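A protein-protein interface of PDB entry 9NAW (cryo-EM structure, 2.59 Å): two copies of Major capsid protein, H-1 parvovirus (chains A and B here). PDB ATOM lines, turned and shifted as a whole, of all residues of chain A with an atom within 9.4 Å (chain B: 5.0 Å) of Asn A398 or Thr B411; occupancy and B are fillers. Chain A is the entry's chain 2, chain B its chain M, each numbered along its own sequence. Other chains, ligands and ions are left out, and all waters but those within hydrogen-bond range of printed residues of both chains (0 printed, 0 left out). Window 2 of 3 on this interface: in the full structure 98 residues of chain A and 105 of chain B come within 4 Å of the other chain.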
ATOM      1  N   VAL A 386     -28.357   0.215 -11.648  1.00  0.00           N
ATOM      2  CA  VAL A 386     -29.547   0.408 -12.467  1.00  0.00           C
ATOM      3  C   VAL A 386     -29.182   0.086 -13.905  1.00  0.00           C
ATOM      4  O   VAL A 386     -28.112   0.477 -14.379  1.00  0.00           O
ATOM      5  CB  VAL A 386     -30.091   1.847 -12.352  1.00  0.00           C
ATOM      6  CG1 VAL A 386     -31.285   2.042 -13.265  1.00  0.00           C
ATOM      7  CG2 VAL A 386     -30.461   2.159 -10.926  1.00  0.00           C
ATOM      8  N   GLN A 387     -30.062  -0.628 -14.598  1.00  0.00           N
ATOM      9  CA  GLN A 387     -29.856  -0.983 -15.992  1.00  0.00           C
ATOM     10  C   GLN A 387     -30.972  -0.403 -16.845  1.00  0.00           C
ATOM     11  O   GLN A 387     -32.051  -0.085 -16.341  1.00  0.00           O
ATOM     12  CB  GLN A 387     -29.805  -2.490 -16.191  1.00  0.00           C
ATOM     13  CG  GLN A 387     -28.639  -3.165 -15.524  1.00  0.00           C
ATOM     14  CD  GLN A 387     -28.648  -4.644 -15.762  1.00  0.00           C
ATOM     15  OE1 GLN A 387     -29.672  -5.216 -16.092  1.00  0.00           O
ATOM     16  NE2 GLN A 387     -27.516  -5.281 -15.556  1.00  0.00           N
ATOM     17  N   SER A 388     -30.701  -0.262 -18.137  1.00  0.00           N
ATOM     18  CA  SER A 388     -31.682   0.288 -19.058  1.00  0.00           C
ATOM     19  C   SER A 388     -32.656  -0.778 -19.536  1.00  0.00           C
ATOM     20  O   SER A 388     -32.298  -1.942 -19.717  1.00  0.00           O
ATOM     21  CB  SER A 388     -30.988   0.912 -20.261  1.00  0.00           C
ATOM     22  OG  SER A 388     -30.263  -0.060 -20.978  1.00  0.00           O
ATOM     23  N   ALA A 389     -33.898  -0.364 -19.737  1.00  0.00           N
ATOM     24  CA  ALA A 389     -34.897  -1.178 -20.413  1.00  0.00           C
ATOM     25  C   ALA A 389     -34.893  -0.876 -21.905  1.00  0.00           C
ATOM     26  O   ALA A 389     -34.724   0.271 -22.295  1.00  0.00           O
ATOM     27  CB  ALA A 389     -36.267  -0.935 -19.828  1.00  0.00           C
ATOM     28  N   SER A 392     -30.660  -5.767 -20.873  1.00  0.00           N
ATOM     29  CA  SER A 392     -29.662  -6.520 -21.614  1.00  0.00           C
ATOM     30  C   SER A 392     -28.693  -7.150 -20.630  1.00  0.00           C
ATOM     31  O   SER A 392     -27.963  -6.442 -19.936  1.00  0.00           O
ATOM     32  CB  SER A 392     -28.908  -5.620 -22.589  1.00  0.00           C
ATOM     33  OG  SER A 392     -29.776  -5.126 -23.588  1.00  0.00           O
ATOM     34  N   PRO A 394     -25.553  -9.781 -20.214  1.00  0.00           N
ATOM     35  CA  PRO A 394     -24.885  -8.704 -19.484  1.00  0.00           C
ATOM     36  C   PRO A 394     -24.980  -7.363 -20.178  1.00  0.00           C
ATOM     37  O   PRO A 394     -24.973  -7.311 -21.400  1.00  0.00           O
ATOM     38  CB  PRO A 394     -23.434  -9.169 -19.444  1.00  0.00           C
ATOM     39  CG  PRO A 394     -23.279  -9.959 -20.661  1.00  0.00           C
ATOM     40  CD  PRO A 394     -24.579 -10.661 -20.876  1.00  0.00           C
ATOM     41  N   PRO A 395     -25.069  -6.288 -19.409  1.00  0.00           N
ATOM     42  CA  PRO A 395     -25.033  -4.954 -20.001  1.00  0.00           C
ATOM     43  C   PRO A 395     -23.616  -4.546 -20.363  1.00  0.00           C
ATOM     44  O   PRO A 395     -22.638  -4.981 -19.757  1.00  0.00           O
ATOM     45  CB  PRO A 395     -25.585  -4.066 -18.885  1.00  0.00           C
ATOM     46  CG  PRO A 395     -25.196  -4.769 -17.659  1.00  0.00           C
ATOM     47  CD  PRO A 395     -25.305  -6.232 -17.961  1.00  0.00           C
ATOM     48  N   ASN A 396     -23.521  -3.691 -21.372  1.00  0.00           N
ATOM     49  CA  ASN A 396     -22.278  -2.998 -21.637  1.00  0.00           C
ATOM     50  C   ASN A 396     -22.212  -1.770 -20.735  1.00  0.00           C
ATOM     51  O   ASN A 396     -23.130  -1.495 -19.961  1.00  0.00           O
ATOM     52  CB  ASN A 396     -22.153  -2.665 -23.124  1.00  0.00           C
ATOM     53  CG  ASN A 396     -23.233  -1.731 -23.623  1.00  0.00           C
ATOM     54  OD1 ASN A 396     -23.685  -0.836 -22.919  1.00  0.00           O
ATOM     55  ND2 ASN A 396     -23.654  -1.942 -24.856  1.00  0.00           N
ATOM     56  N   GLN A 397     -21.120  -1.011 -20.830  1.00  0.00           N
ATOM     57  CA  GLN A 397     -20.925   0.083 -19.884  1.00  0.00           C
ATOM     58  C   GLN A 397     -21.989   1.156 -20.048  1.00  0.00           C
ATOM     59  O   GLN A 397     -22.310   1.870 -19.094  1.00  0.00           O
ATOM     60  CB  GLN A 397     -19.537   0.687 -20.047  1.00  0.00           C
ATOM     61  CG  GLN A 397     -19.315   1.337 -21.379  1.00  0.00           C
ATOM     62  CD  GLN A 397     -17.953   1.957 -21.484  1.00  0.00           C
ATOM     63  OE1 GLN A 397     -17.049   1.616 -20.727  1.00  0.00           O
ATOM     64  NE2 GLN A 397     -17.793   2.876 -22.424  1.00  0.00           N
ATOM     65  N   ASN A 398     -22.550   1.284 -21.248  1.00  0.00           N
ATOM     66  CA  ASN A 398     -23.549   2.319 -21.480  1.00  0.00           C
ATOM     67  C   ASN A 398     -24.927   1.871 -21.026  1.00  0.00           C
ATOM     68  O   ASN A 398     -25.839   2.690 -20.886  1.00  0.00           O
ATOM     69  CB  ASN A 398     -23.567   2.698 -22.955  1.00  0.00           C
ATOM     70  CG  ASN A 398     -22.337   3.455 -23.367  1.00  0.00           C
ATOM     71  OD1 ASN A 398     -21.687   4.091 -22.545  1.00  0.00           O
ATOM     72  ND2 ASN A 398     -21.999   3.383 -24.641  1.00  0.00           N
ATOM     73  N   GLN A 399     -25.105   0.570 -20.803  1.00  0.00           N
ATOM     74  CA  GLN A 399     -26.425   0.059 -20.456  1.00  0.00           C
ATOM     75  C   GLN A 399     -26.610  -0.116 -18.956  1.00  0.00           C
ATOM     76  O   GLN A 399     -27.664  -0.587 -18.520  1.00  0.00           O
ATOM     77  CB  GLN A 399     -26.670  -1.254 -21.185  1.00  0.00           C
ATOM     78  CG  GLN A 399     -26.810  -1.079 -22.670  1.00  0.00           C
ATOM     79  CD  GLN A 399     -26.933  -2.382 -23.396  1.00  0.00           C
ATOM     80  OE1 GLN A 399     -26.457  -3.411 -22.928  1.00  0.00           O
ATOM     81  NE2 GLN A 399     -27.586  -2.355 -24.546  1.00  0.00           N
ATOM     82  N   ILE A 400     -25.618   0.234 -18.152  1.00  0.00           N
ATOM     83  CA  ILE A 400     -25.718   0.101 -16.705  1.00  0.00           C
ATOM     84  C   ILE A 400     -25.246   1.388 -16.053  1.00  0.00           C
ATOM     85  O   ILE A 400     -24.351   2.067 -16.563  1.00  0.00           O
ATOM     86  CB  ILE A 400     -24.913  -1.103 -16.176  1.00  0.00           C
ATOM     87  CG1 ILE A 400     -25.147  -1.271 -14.679  1.00  0.00           C
ATOM     88  CG2 ILE A 400     -23.441  -0.948 -16.481  1.00  0.00           C
ATOM     89  CD1 ILE A 400     -24.638  -2.542 -14.129  1.00  0.00           C
ATOM     90  N   LEU A 401     -25.858   1.724 -14.928  1.00  0.00           N
ATOM     91  CA  LEU A 401     -25.462   2.864 -14.123  1.00  0.00           C
ATOM     92  C   LEU A 401     -25.100   2.345 -12.741  1.00  0.00           C
ATOM     93  O   LEU A 401     -25.949   1.779 -12.046  1.00  0.00           O
ATOM     94  CB  LEU A 401     -26.586   3.889 -14.054  1.00  0.00           C
ATOM     95  CG  LEU A 401     -26.347   5.175 -13.290  1.00  0.00           C
ATOM     96  CD1 LEU A 401     -25.246   5.944 -13.971  1.00  0.00           C
ATOM     97  CD2 LEU A 401     -27.617   5.974 -13.269  1.00  0.00           C
ATOM     98  N   GLN A 402     -23.846   2.529 -12.350  1.00  0.00           N
ATOM     99  CA  GLN A 402     -23.300   1.944 -11.139  1.00  0.00           C
ATOM    100  C   GLN A 402     -22.590   3.032 -10.354  1.00  0.00           C
ATOM    101  O   GLN A 402     -22.369   4.136 -10.852  1.00  0.00           O
ATOM    102  CB  GLN A 402     -22.362   0.788 -11.474  1.00  0.00           C
ATOM    103  CG  GLN A 402     -21.164   1.189 -12.263  1.00  0.00           C
ATOM    104  CD  GLN A 402     -20.349  -0.002 -12.671  1.00  0.00           C
ATOM    105  OE1 GLN A 402     -20.845  -1.120 -12.697  1.00  0.00           O
ATOM    106  NE2 GLN A 402     -19.095   0.226 -13.012  1.00  0.00           N
ATOM    107  N   ASP A 405     -19.969   5.776 -11.243  1.00  0.00           N
ATOM    108  CA  ASP A 405     -20.262   6.748 -12.285  1.00  0.00           C
ATOM    109  C   ASP A 405     -20.476   8.129 -11.680  1.00  0.00           C
ATOM    110  O   ASP A 405     -21.023   8.264 -10.583  1.00  0.00           O
ATOM    111  CB  ASP A 405     -21.503   6.309 -13.052  1.00  0.00           C
ATOM    112  CG  ASP A 405     -21.275   5.044 -13.843  1.00  0.00           C
ATOM    113  OD1 ASP A 405     -20.104   4.680 -14.056  1.00  0.00           O
ATOM    114  OD2 ASP A 405     -22.267   4.403 -14.235  1.00  0.00           O
ATOM    115  N   ASN B 197     -17.939  -4.379 -20.263  1.00  0.00           N
ATOM    116  CA  ASN B 197     -16.813  -3.562 -20.702  1.00  0.00           C
ATOM    117  C   ASN B 197     -15.794  -3.367 -19.589  1.00  0.00           C
ATOM    118  O   ASN B 197     -14.801  -2.657 -19.772  1.00  0.00           O
ATOM    119  CB  ASN B 197     -17.302  -2.206 -21.198  1.00  0.00           C
ATOM    120  CG  ASN B 197     -18.142  -2.312 -22.437  1.00  0.00           C
ATOM    121  OD1 ASN B 197     -19.221  -1.734 -22.515  1.00  0.00           O
ATOM    122  ND2 ASN B 197     -17.649  -3.042 -23.424  1.00  0.00           N
ATOM    123  N   ALA B 406     -28.217  11.669 -21.946  1.00  0.00           N
ATOM    124  CA  ALA B 406     -27.424  10.634 -21.294  1.00  0.00           C
ATOM    125  C   ALA B 406     -27.000  11.066 -19.897  1.00  0.00           C
ATOM    126  O   ALA B 406     -26.355  12.103 -19.731  1.00  0.00           O
ATOM    127  CB  ALA B 406     -26.191  10.296 -22.131  1.00  0.00           C
ATOM    128  N   GLY B 409     -22.862  10.387 -18.585  1.00  0.00           N
ATOM    129  CA  GLY B 409     -22.110  10.012 -19.765  1.00  0.00           C
ATOM    130  C   GLY B 409     -22.277   8.570 -20.171  1.00  0.00           C
ATOM    131  O   GLY B 409     -21.350   7.977 -20.725  1.00  0.00           O
ATOM    132  N   ARG B 410     -23.436   7.984 -19.903  1.00  0.00           N
ATOM    133  CA  ARG B 410     -23.740   6.618 -20.303  1.00  0.00           C
ATOM    134  C   ARG B 410     -24.854   6.668 -21.335  1.00  0.00           C
ATOM    135  O   ARG B 410     -25.958   7.131 -21.035  1.00  0.00           O
ATOM    136  CB  ARG B 410     -24.141   5.769 -19.103  1.00  0.00           C
ATOM    137  CG  ARG B 410     -23.054   5.666 -18.067  1.00  0.00           C
ATOM    138  CD  ARG B 410     -21.845   4.997 -18.658  1.00  0.00           C
ATOM    139  NE  ARG B 410     -20.767   4.846 -17.696  1.00  0.00           N
ATOM    140  CZ  ARG B 410     -19.529   4.503 -18.022  1.00  0.00           C
ATOM    141  NH1 ARG B 410     -19.215   4.294 -19.289  1.00  0.00           N
ATOM    142  NH2 ARG B 410     -18.605   4.378 -17.086  1.00  0.00           N
ATOM    143  N   THR B 411     -24.514   6.343 -22.586  1.00  0.00           N
ATOM    144  CA  THR B 411     -25.462   6.507 -23.721  1.00  0.00           C
ATOM    145  C   THR B 411     -26.880   6.023 -23.415  1.00  0.00           C
ATOM    146  O   THR B 411     -27.823   6.788 -23.687  1.00  0.00           O
ATOM    147  CB  THR B 411     -24.927   5.774 -24.958  1.00  0.00           C
ATOM    148  OG1 THR B 411     -23.647   6.322 -25.270  1.00  0.00           O
ATOM    149  CG2 THR B 411     -25.842   5.891 -26.158  1.00  0.00           C
ATOM    150  N   ASN B 412     -27.033   4.819 -22.873  1.00  0.00           N
ATOM    151  CA  ASN B 412     -28.367   4.261 -22.718  1.00  0.00           C
ATOM    152  C   ASN B 412     -29.010   4.596 -21.385  1.00  0.00           C
ATOM    153  O   ASN B 412     -30.162   4.217 -21.161  1.00  0.00           O
ATOM    154  CB  ASN B 412     -28.330   2.748 -22.903  1.00  0.00           C
ATOM    155  CG  ASN B 412     -28.078   2.350 -24.331  1.00  0.00           C
ATOM    156  OD1 ASN B 412     -28.972   2.420 -25.166  1.00  0.00           O
ATOM    157  ND2 ASN B 412     -26.856   1.934 -24.625  1.00  0.00           N
ATOM    158  N   MET B 413     -28.311   5.288 -20.497  1.00  0.00           N
ATOM    159  CA  MET B 413     -28.881   5.730 -19.234  1.00  0.00           C
ATOM    160  C   MET B 413     -29.569   7.066 -19.426  1.00  0.00           C
ATOM    161  O   MET B 413     -28.997   7.985 -20.015  1.00  0.00           O
ATOM    162  CB  MET B 413     -27.813   5.840 -18.150  1.00  0.00           C
ATOM    163  CG  MET B 413     -27.253   4.521 -17.683  1.00  0.00           C
ATOM    164  SD  MET B 413     -28.531   3.548 -16.878  1.00  0.00           S
ATOM    165  CE  MET B 413     -28.851   2.379 -18.151  1.00  0.00           C
ATOM    166  N   HIS B 414     -30.790   7.169 -18.931  1.00  0.00           N
ATOM    167  CA  HIS B 414     -31.587   8.365 -19.097  1.00  0.00           C
ATOM    168  C   HIS B 414     -32.181   8.707 -17.746  1.00  0.00           C
ATOM    169  O   HIS B 414     -32.321   7.845 -16.880  1.00  0.00           O
ATOM    170  CB  HIS B 414     -32.674   8.145 -20.148  1.00  0.00           C
ATOM    171  CG  HIS B 414     -32.147   7.600 -21.437  1.00  0.00           C
ATOM    172  ND1 HIS B 414     -31.273   8.300 -22.237  1.00  0.00           N
ATOM    173  CD2 HIS B 414     -32.390   6.435 -22.075  1.00  0.00           C
ATOM    174  CE1 HIS B 414     -30.980   7.576 -23.303  1.00  0.00           C
ATOM    175  NE2 HIS B 414     -31.649   6.441 -23.230  1.00  0.00           N
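No position is printed for both chains.
Of the 16 pairs that touch across the chains among the printed residues, none has its exchanged pair printed and touching as well.
NH2 of Arg B410 is in salt-bridge range of OD1 of Asp A405 (3.4 Å).
OD1 of Asn B197 sits at hydrogen-bond distance from N of Gln A397 (2.6 Å).
SD of Met B413 sits close to N of Leu A401 (3.8 Å).
O of Asn A398 lies within hydrogen-bond range of N of Asn B412 (3.1 Å).
OG1 of Thr B411 is in hydrogen-bond range of ND2 of Asn A398 (3.4 Å).
Hydrophobic or aromatic side chains of chain B within 4 Å of the printed part of chain A: Met B413.
Printed residues of chain A that touch a printed residue of chain B: Val A386, Gln A387, Ser A388, Asn A396, Gln A397, Asn A398, Gln A399, Ile A400, Leu A401 and Asp A405.
Hydrophobic or aromatic side chains of chain A that line the printed part of chain B: Leu A401.
Among the printed residues, 16 pairs touch across the chains.
Asn A398 touches just these residues of chain B: Arg B410, Thr B411, Asn B412 and Met B413.
Of chain A, only Ser A388, Asn A398 and Gln A399 come within 4 Å of Asn B412.
Printed residues of chain B within 4 Å of Ser A388: Asn B412 and Met B413.
Of the printed residues of chain A, Arg B410 touches Gln A397, Asn A398 and Asp A405.
Of the printed residues of chain B, Ile A400 touches Met B413 (3.9 Å).
Of the printed residues of chain B, Val A386 touches Met B413.
Of the printed residues of chain B, Asp A405 touches Arg B410.
Ala A389 touches none of the printed residues of chain B.
His B414 touches none of the printed residues of chain A.
The nearest residue of chain B that does not touch Asn A398 is Gly B409 (4.3 Å).
The nearest printed residue of chain A that does not touch Thr B411 is Gln A399 (6.1 Å).
The nearest printed residue of chain A that does not touch Met B413 is Gln A397 (5.8 Å).
Among the printed residues, pairs that only touch across the chains: Val A386 with Met B413, Gln A387 with Met B413, Ser A388 with Asn B412, Ser A388 with Met B413, Asn A396 with Asn B197, Gln A397 with Arg B410, Asn A398 with Arg B410, Asn A398 with Met B413, Gln A399 with Asn B412, Gln A399 with Met B413 and Ile A400 with Met B413.
The side-chain amide oxygen (OD1) of Asn A396 sits at hydrogen-bond distance from the backbone NH (N) of Gln A399.
The backbone NH (N) of Asn A398 sits at hydrogen-bond distance from the side-chain amide oxygen (OD1) of Asn A396, at 2.9 Å.
A ring nitrogen (NE2) of His B414 lies close to the backbone carbonyl oxygen (O) of Asn B412 (3.4 Å).
The backbone carbonyl oxygen (O) of Gln A399 is in hydrogen-bond range of the backbone NH (N) of Ser A388.
The side-chain carboxylate (OD2) of Asp A405 sits at hydrogen-bond distance from the backbone NH (N) of Gln A402 (3.1 Å).
The backbone NH of Leu A401 lies within hydrogen-bond range of the backbone carbonyl oxygen of Val A386 (2.6 Å).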
